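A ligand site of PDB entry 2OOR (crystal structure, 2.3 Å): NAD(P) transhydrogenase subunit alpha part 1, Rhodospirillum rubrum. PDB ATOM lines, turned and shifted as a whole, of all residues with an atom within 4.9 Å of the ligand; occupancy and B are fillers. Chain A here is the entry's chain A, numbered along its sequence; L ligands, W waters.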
ATOM      1  N   PRO A 126     -15.461 -23.037  35.721  1.00  0.00           N
ATOM      2  CA  PRO A 126     -16.440 -21.956  35.595  1.00  0.00           C
ATOM      3  C   PRO A 126     -15.758 -20.595  35.431  1.00  0.00           C
ATOM      4  O   PRO A 126     -14.760 -20.319  36.091  1.00  0.00           O
ATOM      5  CB  PRO A 126     -17.227 -22.019  36.910  1.00  0.00           C
ATOM      6  CG  PRO A 126     -16.351 -22.732  37.854  1.00  0.00           C
ATOM      7  CD  PRO A 126     -15.556 -23.701  37.038  1.00  0.00           C
ATOM      8  N   ARG A 127     -16.306 -19.764  34.542  1.00  0.00           N
ATOM      9  CA  ARG A 127     -15.683 -18.484  34.183  1.00  0.00           C
ATOM     10  C   ARG A 127     -16.023 -17.399  35.212  1.00  0.00           C
ATOM     11  O   ARG A 127     -16.861 -16.526  34.952  1.00  0.00           O
ATOM     12  CB  ARG A 127     -16.118 -18.076  32.774  1.00  0.00           C
ATOM     13  CG  ARG A 127     -15.864 -19.149  31.724  1.00  0.00           C
ATOM     14  CD  ARG A 127     -15.640 -18.549  30.330  1.00  0.00           C
ATOM     15  NE  ARG A 127     -15.966 -19.506  29.254  1.00  0.00           N
ATOM     16  CZ  ARG A 127     -15.517 -19.444  27.996  1.00  0.00           C
ATOM     17  NH1 ARG A 127     -14.699 -18.467  27.584  1.00  0.00           N
ATOM     18  NH2 ARG A 127     -15.897 -20.379  27.125  1.00  0.00           N
ATOM     19  N   ILE A 128     -15.357 -17.463  36.361  1.00  0.00           N
ATOM     20  CA  ILE A 128     -15.543 -16.522  37.475  1.00  0.00           C
ATOM     21  C   ILE A 128     -14.225 -15.844  37.832  1.00  0.00           C
ATOM     22  O   ILE A 128     -13.175 -16.501  37.856  1.00  0.00           O
ATOM     23  CB  ILE A 128     -16.174 -17.205  38.732  1.00  0.00           C
ATOM     24  CG1 ILE A 128     -15.363 -18.437  39.179  1.00  0.00           C
ATOM     25  CG2 ILE A 128     -17.635 -17.585  38.436  1.00  0.00           C
ATOM     26  CD1 ILE A 128     -15.819 -19.071  40.492  1.00  0.00           C
ATOM     27  N   SER A 129     -14.271 -14.546  38.138  1.00  0.00           N
ATOM     28  CA  SER A 129     -13.060 -13.710  38.258  1.00  0.00           C
ATOM     29  C   SER A 129     -11.999 -14.229  39.247  1.00  0.00           C
ATOM     30  O   SER A 129     -10.804 -14.058  39.004  1.00  0.00           O
ATOM     31  CB  SER A 129     -13.434 -12.267  38.624  1.00  0.00           C
ATOM     32  OG  SER A 129     -12.351 -11.388  38.391  1.00  0.00           O
ATOM     33  N   ALA A 131     -11.472 -17.392  39.753  1.00  0.00           N
ATOM     34  CA  ALA A 131     -10.902 -18.575  39.088  1.00  0.00           C
ATOM     35  C   ALA A 131     -10.001 -18.262  37.875  1.00  0.00           C
ATOM     36  O   ALA A 131      -9.580 -19.189  37.192  1.00  0.00           O
ATOM     37  CB  ALA A 131     -12.027 -19.534  38.682  1.00  0.00           C
ATOM     38  N   GLN A 132      -9.723 -16.988  37.596  1.00  0.00           N
ATOM     39  CA  GLN A 132      -8.698 -16.602  36.594  1.00  0.00           C
ATOM     40  C   GLN A 132      -7.313 -17.165  36.907  1.00  0.00           C
ATOM     41  O   GLN A 132      -6.562 -17.524  36.000  1.00  0.00           O
ATOM     42  CB  GLN A 132      -8.607 -15.067  36.460  1.00  0.00           C
ATOM     43  CG  GLN A 132      -9.704 -14.450  35.588  1.00  0.00           C
ATOM     44  CD  GLN A 132      -9.761 -12.925  35.684  1.00  0.00           C
ATOM     45  OE1 GLN A 132      -9.482 -12.334  36.734  1.00  0.00           O
ATOM     46  NE2 GLN A 132     -10.151 -12.283  34.583  1.00  0.00           N
ATOM     47  N   ASP A 135      -7.419 -20.906  35.704  1.00  0.00           N
ATOM     48  CA  ASP A 135      -8.046 -21.100  34.384  1.00  0.00           C
ATOM     49  C   ASP A 135      -6.999 -21.417  33.310  1.00  0.00           C
ATOM     50  O   ASP A 135      -6.238 -20.543  32.901  1.00  0.00           O
ATOM     51  CB  ASP A 135      -8.823 -19.833  33.991  1.00  0.00           C
ATOM     52  CG  ASP A 135      -9.525 -19.949  32.646  1.00  0.00           C
ATOM     53  OD1 ASP A 135      -9.973 -21.051  32.274  1.00  0.00           O
ATOM     54  OD2 ASP A 135      -9.642 -18.912  31.965  1.00  0.00           O
ATOM     55  N   SER A 138      -7.216 -19.421  29.625  1.00  0.00           N
ATOM     56  CA  SER A 138      -6.618 -18.086  29.563  1.00  0.00           C
ATOM     57  C   SER A 138      -5.092 -18.083  29.546  1.00  0.00           C
ATOM     58  O   SER A 138      -4.478 -17.360  28.762  1.00  0.00           O
ATOM     59  CB  SER A 138      -7.124 -17.224  30.722  1.00  0.00           C
ATOM     60  OG  SER A 138      -8.482 -16.877  30.536  1.00  0.00           O
ATOM     61  N   GLY A 179     -11.359 -11.642  16.135  1.00  0.00           N
ATOM     62  CA  GLY A 179     -11.674 -12.172  17.464  1.00  0.00           C
ATOM     63  C   GLY A 179     -10.649 -11.708  18.479  1.00  0.00           C
ATOM     64  O   GLY A 179      -9.484 -12.109  18.409  1.00  0.00           O
ATOM     65  N   VAL A 180     -11.092 -10.870  19.418  1.00  0.00           N
ATOM     66  CA  VAL A 180     -10.233 -10.239  20.418  1.00  0.00           C
ATOM     67  C   VAL A 180     -10.634 -10.768  21.793  1.00  0.00           C
ATOM     68  O   VAL A 180     -11.228 -10.063  22.622  1.00  0.00           O
ATOM     69  CB  VAL A 180     -10.331  -8.683  20.333  1.00  0.00           C
ATOM     70  CG1 VAL A 180      -9.362  -8.003  21.304  1.00  0.00           C
ATOM     71  CG2 VAL A 180     -10.043  -8.208  18.909  1.00  0.00           C
ATOM     72  N   GLY A 181     -10.309 -12.036  22.018  1.00  0.00           N
ATOM     73  CA  GLY A 181     -10.379 -12.652  23.338  1.00  0.00           C
ATOM     74  C   GLY A 181      -9.003 -12.552  23.980  1.00  0.00           C
ATOM     75  O   GLY A 181      -8.290 -11.569  23.761  1.00  0.00           O
ATOM     76  N   VAL A 182      -8.622 -13.571  24.748  1.00  0.00           N
ATOM     77  CA  VAL A 182      -7.337 -13.571  25.441  1.00  0.00           C
ATOM     78  C   VAL A 182      -6.176 -13.670  24.446  1.00  0.00           C
ATOM     79  O   VAL A 182      -5.184 -12.949  24.562  1.00  0.00           O
ATOM     80  CB  VAL A 182      -7.264 -14.727  26.487  1.00  0.00           C
ATOM     81  CG1 VAL A 182      -5.884 -14.789  27.150  1.00  0.00           C
ATOM     82  CG2 VAL A 182      -8.341 -14.559  27.562  1.00  0.00           C
ATOM     83  N   ALA A 183      -6.316 -14.549  23.457  1.00  0.00           N
ATOM     84  CA  ALA A 183      -5.303 -14.737  22.408  1.00  0.00           C
ATOM     85  C   ALA A 183      -5.193 -13.536  21.476  1.00  0.00           C
ATOM     86  O   ALA A 183      -4.095 -13.085  21.169  1.00  0.00           O
ATOM     87  CB  ALA A 183      -5.599 -15.995  21.611  1.00  0.00           C
ATOM     88  N   THR A 201     -11.289  -6.905  14.948  1.00  0.00           N
ATOM     89  CA  THR A 201     -12.740  -6.986  14.991  1.00  0.00           C
ATOM     90  C   THR A 201     -13.211  -8.135  15.873  1.00  0.00           C
ATOM     91  O   THR A 201     -12.487  -9.110  16.100  1.00  0.00           O
ATOM     92  CB  THR A 201     -13.346  -7.142  13.568  1.00  0.00           C
ATOM     93  OG1 THR A 201     -14.753  -6.925  13.627  1.00  0.00           O
ATOM     94  CG2 THR A 201     -13.047  -8.525  12.963  1.00  0.00           C
ATOM     95  N   ASP A 202     -14.441  -8.007  16.365  1.00  0.00           N
ATOM     96  CA  ASP A 202     -15.080  -8.981  17.239  1.00  0.00           C
ATOM     97  C   ASP A 202     -16.585  -8.701  17.241  1.00  0.00           C
ATOM     98  O   ASP A 202     -17.025  -7.625  16.817  1.00  0.00           O
ATOM     99  CB  ASP A 202     -14.544  -8.828  18.663  1.00  0.00           C
ATOM    100  CG  ASP A 202     -14.679 -10.098  19.502  1.00  0.00           C
ATOM    101  OD1 ASP A 202     -15.810 -10.602  19.678  1.00  0.00           O
ATOM    102  OD2 ASP A 202     -13.653 -10.586  20.006  1.00  0.00           O
ATOM    103  N   VAL A 203     -17.353  -9.683  17.713  1.00  0.00           N
ATOM    104  CA  VAL A 203     -18.804  -9.517  17.908  1.00  0.00           C
ATOM    105  C   VAL A 203     -19.174  -8.813  19.223  1.00  0.00           C
ATOM    106  O   VAL A 203     -20.217  -8.168  19.301  1.00  0.00           O
ATOM    107  CB  VAL A 203     -19.562 -10.877  17.828  1.00  0.00           C
ATOM    108  CG1 VAL A 203     -19.328 -11.529  16.472  1.00  0.00           C
ATOM    109  CG2 VAL A 203     -19.183 -11.847  18.972  1.00  0.00           C
ATOM    110  N   ARG A 204     -18.324  -8.932  20.250  1.00  0.00           N
ATOM    111  CA  ARG A 204     -18.580  -8.328  21.552  1.00  0.00           C
ATOM    112  C   ARG A 204     -18.282  -6.829  21.543  1.00  0.00           C
ATOM    113  O   ARG A 204     -17.310  -6.388  20.921  1.00  0.00           O
ATOM    114  CB  ARG A 204     -17.782  -9.045  22.651  1.00  0.00           C
ATOM    115  CG  ARG A 204     -18.119 -10.537  22.750  1.00  0.00           C
ATOM    116  CD  ARG A 204     -17.551 -11.227  23.974  1.00  0.00           C
ATOM    117  NE  ARG A 204     -16.081 -11.291  23.997  1.00  0.00           N
ATOM    118  CZ  ARG A 204     -15.261 -10.428  24.609  1.00  0.00           C
ATOM    119  NH1 ARG A 204     -15.717  -9.375  25.304  1.00  0.00           N
ATOM    120  NH2 ARG A 204     -13.940 -10.625  24.536  1.00  0.00           N
ATOM    121  N   GLY A 234     -19.806 -14.908  29.358  1.00  0.00           N
ATOM    122  CA  GLY A 234     -18.792 -14.068  28.699  1.00  0.00           C
ATOM    123  C   GLY A 234     -18.309 -14.531  27.330  1.00  0.00           C
ATOM    124  O   GLY A 234     -17.416 -13.906  26.759  1.00  0.00           O
ATOM    125  N   TYR A 235     -18.911 -15.588  26.789  1.00  0.00           N
ATOM    126  CA  TYR A 235     -18.480 -16.177  25.506  1.00  0.00           C
ATOM    127  C   TYR A 235     -19.441 -15.785  24.389  1.00  0.00           C
ATOM    128  O   TYR A 235     -20.557 -15.319  24.644  1.00  0.00           O
ATOM    129  CB  TYR A 235     -18.312 -17.713  25.601  1.00  0.00           C
ATOM    130  CG  TYR A 235     -19.308 -18.453  26.479  1.00  0.00           C
ATOM    131  CD1 TYR A 235     -19.038 -18.694  27.822  1.00  0.00           C
ATOM    132  CD2 TYR A 235     -20.527 -18.909  25.956  1.00  0.00           C
ATOM    133  CE1 TYR A 235     -19.951 -19.366  28.628  1.00  0.00           C
ATOM    134  CE2 TYR A 235     -21.450 -19.582  26.763  1.00  0.00           C
ATOM    135  CZ  TYR A 235     -21.152 -19.814  28.095  1.00  0.00           C
ATOM    136  OH  TYR A 235     -22.046 -20.483  28.897  1.00  0.00           O
ATOM    137  N   ALA A 236     -19.001 -15.954  23.141  1.00  0.00           N
ATOM    138  CA  ALA A 236     -19.786 -15.549  21.978  1.00  0.00           C
ATOM    139  C   ALA A 236     -20.843 -16.593  21.608  1.00  0.00           C
ATOM    140  O   ALA A 236     -20.770 -17.749  22.026  1.00  0.00           O
ATOM    141  CB  ALA A 236     -18.884 -15.290  20.789  1.00  0.00           C
ATOM    142  N   MET A 239     -23.881 -15.890  15.313  1.00  0.00           N
ATOM    143  CA  MET A 239     -24.470 -14.612  14.895  1.00  0.00           C
ATOM    144  C   MET A 239     -25.408 -14.714  13.693  1.00  0.00           C
ATOM    145  O   MET A 239     -26.265 -13.856  13.502  1.00  0.00           O
ATOM    146  CB  MET A 239     -23.369 -13.609  14.560  1.00  0.00           C
ATOM    147  CG  MET A 239     -22.470 -13.242  15.737  1.00  0.00           C
ATOM    148  SD  MET A 239     -23.298 -12.237  16.977  1.00  0.00           S
ATOM    149  CE  MET A 239     -23.262 -10.619  16.200  1.00  0.00           C
ATOM    150  N   PHE A 243     -25.321 -11.391   9.470  1.00  0.00           N
ATOM    151  CA  PHE A 243     -24.185 -10.714  10.110  1.00  0.00           C
ATOM    152  C   PHE A 243     -22.849 -11.123   9.464  1.00  0.00           C
ATOM    153  O   PHE A 243     -21.944 -10.304   9.357  1.00  0.00           O
ATOM    154  CB  PHE A 243     -24.130 -10.993  11.617  1.00  0.00           C
ATOM    155  CG  PHE A 243     -22.962 -10.352  12.310  1.00  0.00           C
ATOM    156  CD1 PHE A 243     -21.765 -11.038  12.479  1.00  0.00           C
ATOM    157  CD2 PHE A 243     -23.048  -9.037  12.777  1.00  0.00           C
ATOM    158  CE1 PHE A 243     -20.683 -10.428  13.109  1.00  0.00           C
ATOM    159  CE2 PHE A 243     -21.974  -8.434  13.416  1.00  0.00           C
ATOM    160  CZ  PHE A 243     -20.787  -9.137  13.575  1.00  0.00           C
ATOM    161  N   GLN A 247     -20.309  -8.418   8.184  1.00  0.00           N
ATOM    162  CA  GLN A 247     -18.948  -8.425   8.702  1.00  0.00           C
ATOM    163  C   GLN A 247     -17.923  -8.565   7.572  1.00  0.00           C
ATOM    164  O   GLN A 247     -16.996  -7.757   7.465  1.00  0.00           O
ATOM    165  CB  GLN A 247     -18.781  -9.574   9.693  1.00  0.00           C
ATOM    166  CG  GLN A 247     -17.451  -9.624  10.439  1.00  0.00           C
ATOM    167  CD  GLN A 247     -17.303 -10.870  11.289  1.00  0.00           C
ATOM    168  OE1 GLN A 247     -17.075 -10.783  12.503  1.00  0.00           O
ATOM    169  NE2 GLN A 247     -17.444 -12.027  10.664  1.00  0.00           N
ATOM    170  N   THR A 264      -8.766 -16.029  15.645  1.00  0.00           N
ATOM    171  CA  THR A 264      -8.822 -16.664  16.973  1.00  0.00           C
ATOM    172  C   THR A 264     -10.236 -17.032  17.428  1.00  0.00           C
ATOM    173  O   THR A 264     -10.421 -17.431  18.581  1.00  0.00           O
ATOM    174  CB  THR A 264      -8.230 -15.707  18.060  1.00  0.00           C
ATOM    175  OG1 THR A 264      -9.216 -14.751  18.461  1.00  0.00           O
ATOM    176  CG2 THR A 264      -6.987 -14.952  17.560  1.00  0.00           C
ATOM    177  N   ALA A 265     -11.227 -16.913  16.549  1.00  0.00           N
ATOM    178  CA  ALA A 265     -12.634 -16.918  16.963  1.00  0.00           C
ATOM    179  C   ALA A 265     -13.155 -18.328  17.267  1.00  0.00           C
ATOM    180  O   ALA A 265     -12.978 -19.238  16.467  1.00  0.00           O
ATOM    181  CB  ALA A 265     -13.498 -16.254  15.918  1.00  0.00           C
ATOM    182  N   LEU A 266     -13.802 -18.463  18.432  1.00  0.00           N
ATOM    183  CA  LEU A 266     -14.334 -19.738  18.924  1.00  0.00           C
ATOM    184  C   LEU A 266     -15.775 -19.539  19.431  1.00  0.00           C
ATOM    185  O   LEU A 266     -16.134 -18.446  19.854  1.00  0.00           O
ATOM    186  CB  LEU A 266     -13.464 -20.255  20.074  1.00  0.00           C
ATOM    187  CG  LEU A 266     -12.390 -21.327  19.818  1.00  0.00           C
ATOM    188  CD1 LEU A 266     -11.354 -20.892  18.799  1.00  0.00           C
ATOM    189  CD2 LEU A 266     -11.701 -21.674  21.135  1.00  0.00           C
ATOM    190  N   ILE A 267     -16.581 -20.600  19.364  1.00  0.00           N
ATOM    191  CA  ILE A 267     -17.944 -20.612  19.926  1.00  0.00           C
ATOM    192  C   ILE A 267     -18.137 -21.967  20.642  1.00  0.00           C
ATOM    193  O   ILE A 267     -18.107 -23.003  19.975  1.00  0.00           O
ATOM    194  CB  ILE A 267     -19.055 -20.434  18.842  1.00  0.00           C
ATOM    195  CG1 ILE A 267     -18.846 -19.140  18.040  1.00  0.00           C
ATOM    196  CG2 ILE A 267     -20.451 -20.399  19.508  1.00  0.00           C
ATOM    197  CD1 ILE A 267     -19.789 -18.958  16.855  1.00  0.00           C
ATOM    198  N   PRO A 268     -18.306 -21.973  21.986  1.00  0.00           N
ATOM    199  CA  PRO A 268     -18.456 -23.237  22.732  1.00  0.00           C
ATOM    200  C   PRO A 268     -19.568 -24.165  22.233  1.00  0.00           C
ATOM    201  O   PRO A 268     -20.671 -23.716  21.932  1.00  0.00           O
ATOM    202  CB  PRO A 268     -18.780 -22.765  24.145  1.00  0.00           C
ATOM    203  CG  PRO A 268     -18.146 -21.441  24.253  1.00  0.00           C
ATOM    204  CD  PRO A 268     -18.336 -20.812  22.906  1.00  0.00           C
ATOM    205  N   PRO A 273     -16.425 -20.184  13.732  1.00  0.00           N
ATOM    206  CA  PRO A 273     -17.107 -19.451  12.667  1.00  0.00           C
ATOM    207  C   PRO A 273     -16.172 -19.103  11.509  1.00  0.00           C
ATOM    208  O   PRO A 273     -15.026 -18.724  11.743  1.00  0.00           O
ATOM    209  CB  PRO A 273     -17.581 -18.182  13.371  1.00  0.00           C
ATOM    210  CG  PRO A 273     -16.596 -17.962  14.447  1.00  0.00           C
ATOM    211  CD  PRO A 273     -16.190 -19.341  14.911  1.00  0.00           C
ATOM    212  N   LEU A 275     -14.603 -16.854   9.105  1.00  0.00           N
ATOM    213  CA  LEU A 275     -14.365 -15.403   8.988  1.00  0.00           C
ATOM    214  C   LEU A 275     -13.596 -14.987   7.731  1.00  0.00           C
ATOM    215  O   LEU A 275     -13.677 -13.830   7.329  1.00  0.00           O
ATOM    216  CB  LEU A 275     -13.648 -14.894  10.236  1.00  0.00           C
ATOM    217  CG  LEU A 275     -14.264 -15.287  11.586  1.00  0.00           C
ATOM    218  CD1 LEU A 275     -13.514 -14.633  12.705  1.00  0.00           C
ATOM    219  CD2 LEU A 275     -15.744 -14.922  11.694  1.00  0.00           C
HETATM  220  P1  LIG L   1     -13.028 -17.367  22.818  1.00  0.00           P
HETATM  221  O1  LIG L   1     -11.809 -18.198  22.865  1.00  0.00           O
HETATM  222  O2  LIG L   1     -14.227 -18.204  23.058  1.00  0.00           O
HETATM  223  O3  LIG L   1     -13.164 -16.618  21.393  1.00  0.00           O
HETATM  224  C1  LIG L   1     -12.332 -15.546  21.021  1.00  0.00           C
HETATM  225  C2  LIG L   1     -13.118 -14.349  20.505  1.00  0.00           C
HETATM  226  O4  LIG L   1     -13.757 -14.653  19.284  1.00  0.00           O
HETATM  227  C3  LIG L   1     -14.219 -13.851  21.446  1.00  0.00           C
HETATM  228  O5  LIG L   1     -13.887 -12.560  21.894  1.00  0.00           O
HETATM  229  C4  LIG L   1     -15.475 -13.865  20.586  1.00  0.00           C
HETATM  230  O6  LIG L   1     -16.308 -12.762  20.842  1.00  0.00           O
HETATM  231  C5  LIG L   1     -14.892 -13.834  19.171  1.00  0.00           C
HETATM  232  N1  LIG L   1     -15.807 -14.275  18.096  1.00  0.00           N
HETATM  233  C6  LIG L   1     -16.641 -15.368  18.088  1.00  0.00           C
HETATM  234  N2  LIG L   1     -17.300 -15.386  16.916  1.00  0.00           N
HETATM  235  C7  LIG L   1     -16.908 -14.337  16.169  1.00  0.00           C
HETATM  236  C8  LIG L   1     -17.277 -13.891  14.897  1.00  0.00           C
HETATM  237  N3  LIG L   1     -18.340 -14.442  14.306  1.00  0.00           N
HETATM  238  N4  LIG L   1     -16.698 -12.757  14.380  1.00  0.00           N
HETATM  239  C9  LIG L   1     -15.755 -12.050  15.126  1.00  0.00           C
HETATM  240  N5  LIG L   1     -15.410 -12.496  16.379  1.00  0.00           N
HETATM  241  C10 LIG L   1     -15.968 -13.619  16.899  1.00  0.00           C
HETATM  242  O7  LIG L   1     -12.967 -16.128  23.872  1.00  0.00           O
HETATM  243  P2  LIG L   1     -12.028 -16.068  25.183  1.00  0.00           P
HETATM  244  O8  LIG L   1     -10.635 -15.805  24.770  1.00  0.00           O
HETATM  245  O9  LIG L   1     -12.297 -17.259  26.011  1.00  0.00           O
HETATM  246  O10 LIG L   1     -12.566 -14.761  25.968  1.00  0.00           O
HETATM  247  C11 LIG L   1     -13.841 -14.183  25.791  1.00  0.00           C
HETATM  248  C12 LIG L   1     -14.249 -13.321  26.989  1.00  0.00           C
HETATM  249  O11 LIG L   1     -14.523 -14.166  28.105  1.00  0.00           O
HETATM  250  C13 LIG L   1     -13.187 -12.324  27.425  1.00  0.00           C
HETATM  251  O12 LIG L   1     -13.761 -11.056  27.650  1.00  0.00           O
HETATM  252  C14 LIG L   1     -12.645 -12.892  28.718  1.00  0.00           C
HETATM  253  O13 LIG L   1     -12.265 -11.898  29.644  1.00  0.00           O
HETATM  254  C15 LIG L   1     -13.803 -13.724  29.241  1.00  0.00           C
HETATM  255  N6  LIG L   1     -13.327 -14.849  30.074  1.00  0.00           N
HETATM  256  C16 LIG L   1     -13.556 -14.849  31.424  1.00  0.00           C
HETATM  257  C17 LIG L   1     -13.114 -15.904  32.227  1.00  0.00           C
HETATM  258  C18 LIG L   1     -13.311 -15.842  33.715  1.00  0.00           C
HETATM  259  O14 LIG L   1     -14.193 -14.891  34.264  1.00  0.00           O
HETATM  260  N7  LIG L   1     -12.660 -16.689  34.529  1.00  0.00           N
HETATM  261  C19 LIG L   1     -12.427 -16.972  31.629  1.00  0.00           C
HETATM  262  C20 LIG L   1     -12.184 -16.945  30.257  1.00  0.00           C
HETATM  263  C21 LIG L   1     -12.643 -15.887  29.485  1.00  0.00           C
HETATM  264  O   HOH W   1     -20.023 -15.678  16.300  1.00  0.00           O
HETATM  265  O   HOH W   2     -16.590 -16.957  22.397  1.00  0.00           O
HETATM  266  O   HOH W   3      -8.947 -18.017  26.409  1.00  0.00           O
HETATM  267  O   HOH W   4      -9.063 -14.418  21.052  1.00  0.00           O
HETATM  268  O   HOH W   5      -8.806 -16.201  22.984  1.00  0.00           O
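The side-chain carboxylate of Asp 202 is in hydrogen-bond range of an oxygen (O6) of the ligand.
OE1 of Gln 247 sits close to N4 of the ligand (2.7 Å).
The backbone NH (N) of Val 182 is in hydrogen-bond range of an oxygen (O8) of the ligand, 3.0 Å away.
The guanidinium group (NH1) of Arg 127 is in salt-bridge range of an oxygen (O9) of the ligand.
An oxygen (O12) of the ligand is in hydrogen-bond range of the guanidinium group (NH2) of Arg 204 (3.1 Å).
A nitrogen (N7) of the ligand lies within hydrogen-bond range of the backbone carbonyl oxygen of Ile 128.
The side-chain carboxylate (OD1) of Asp 202 sits at hydrogen-bond distance from the backbone NH (N) of Arg 204, 3.1 Å away.
The side-chain carboxylate (OD2) of Asp 202 is in hydrogen-bond range of the backbone NH (N) of Val 180 (2.6 Å).
NH2 of Arg 204 lies within hydrogen-bond range of O of Val 180.
OG of Ser 138 sits at hydrogen-bond distance from OD2 of Asp 135.
OG1 of Thr 264 sits at hydrogen-bond distance from O of Gly 179.
N of Gly 179 lies within hydrogen-bond range of O of Thr 201 (2.8 Å).
OE1 of Gln 132 lies close to O of Ser 129 (3.1 Å).
The backbone carbonyl oxygen (O) of Gly 234 lies close to an oxygen (O11) of the ligand (3.2 Å).
Residues that only touch the ligand: Ser 129 (3.9 Å), Gln 132 (3.9 Å), Asp 135 (3.4 Å), Ser 138 (3.7 Å), Gly 179 (3.7 Å), Val 180 (3.7 Å), Gly 181 (3.5 Å), Val 203 (3.5 Å), Ala 236 (3.5 Å), Thr 264 (3.6 Å), Ala 265 (3.4 Å), Leu 266 (3.5 Å), Pro 273 (3.6 Å) and Leu 275 (3.6 Å).
Hydrophobic or aromatic side chains that line the ligand: Val 182, Val 203, Ala 236, Ala 265, Leu 266, Pro 273 and Leu 275.
Within 4 Å of the ligand: Arg 127, Ile 128, Ser 129, Gln 132, Asp 135, Ser 138, Gly 179, Val 180, Gly 181, Val 182, Asp 202, Val 203, Arg 204, Gly 234, Ala 236, Gln 247, Thr 264, Ala 265, Leu 266, Pro 273 and Leu 275.
Water W5 lies within hydrogen-bond range of O8 of the ligand (2.6 Å), N of Ala 183 (3.0 Å) and N of Val 182 (3.2 Å).
Water W2 lies within hydrogen-bond range of the backbone NH (N) of Ala 236, an oxygen (O2) of the ligand and the backbone carbonyl oxygen (O) of Leu 266.
Water W4 lies within hydrogen-bond range of the side-chain hydroxyl of Thr 264 (2.6 Å) and the backbone NH of Gly 181 (2.9 Å).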
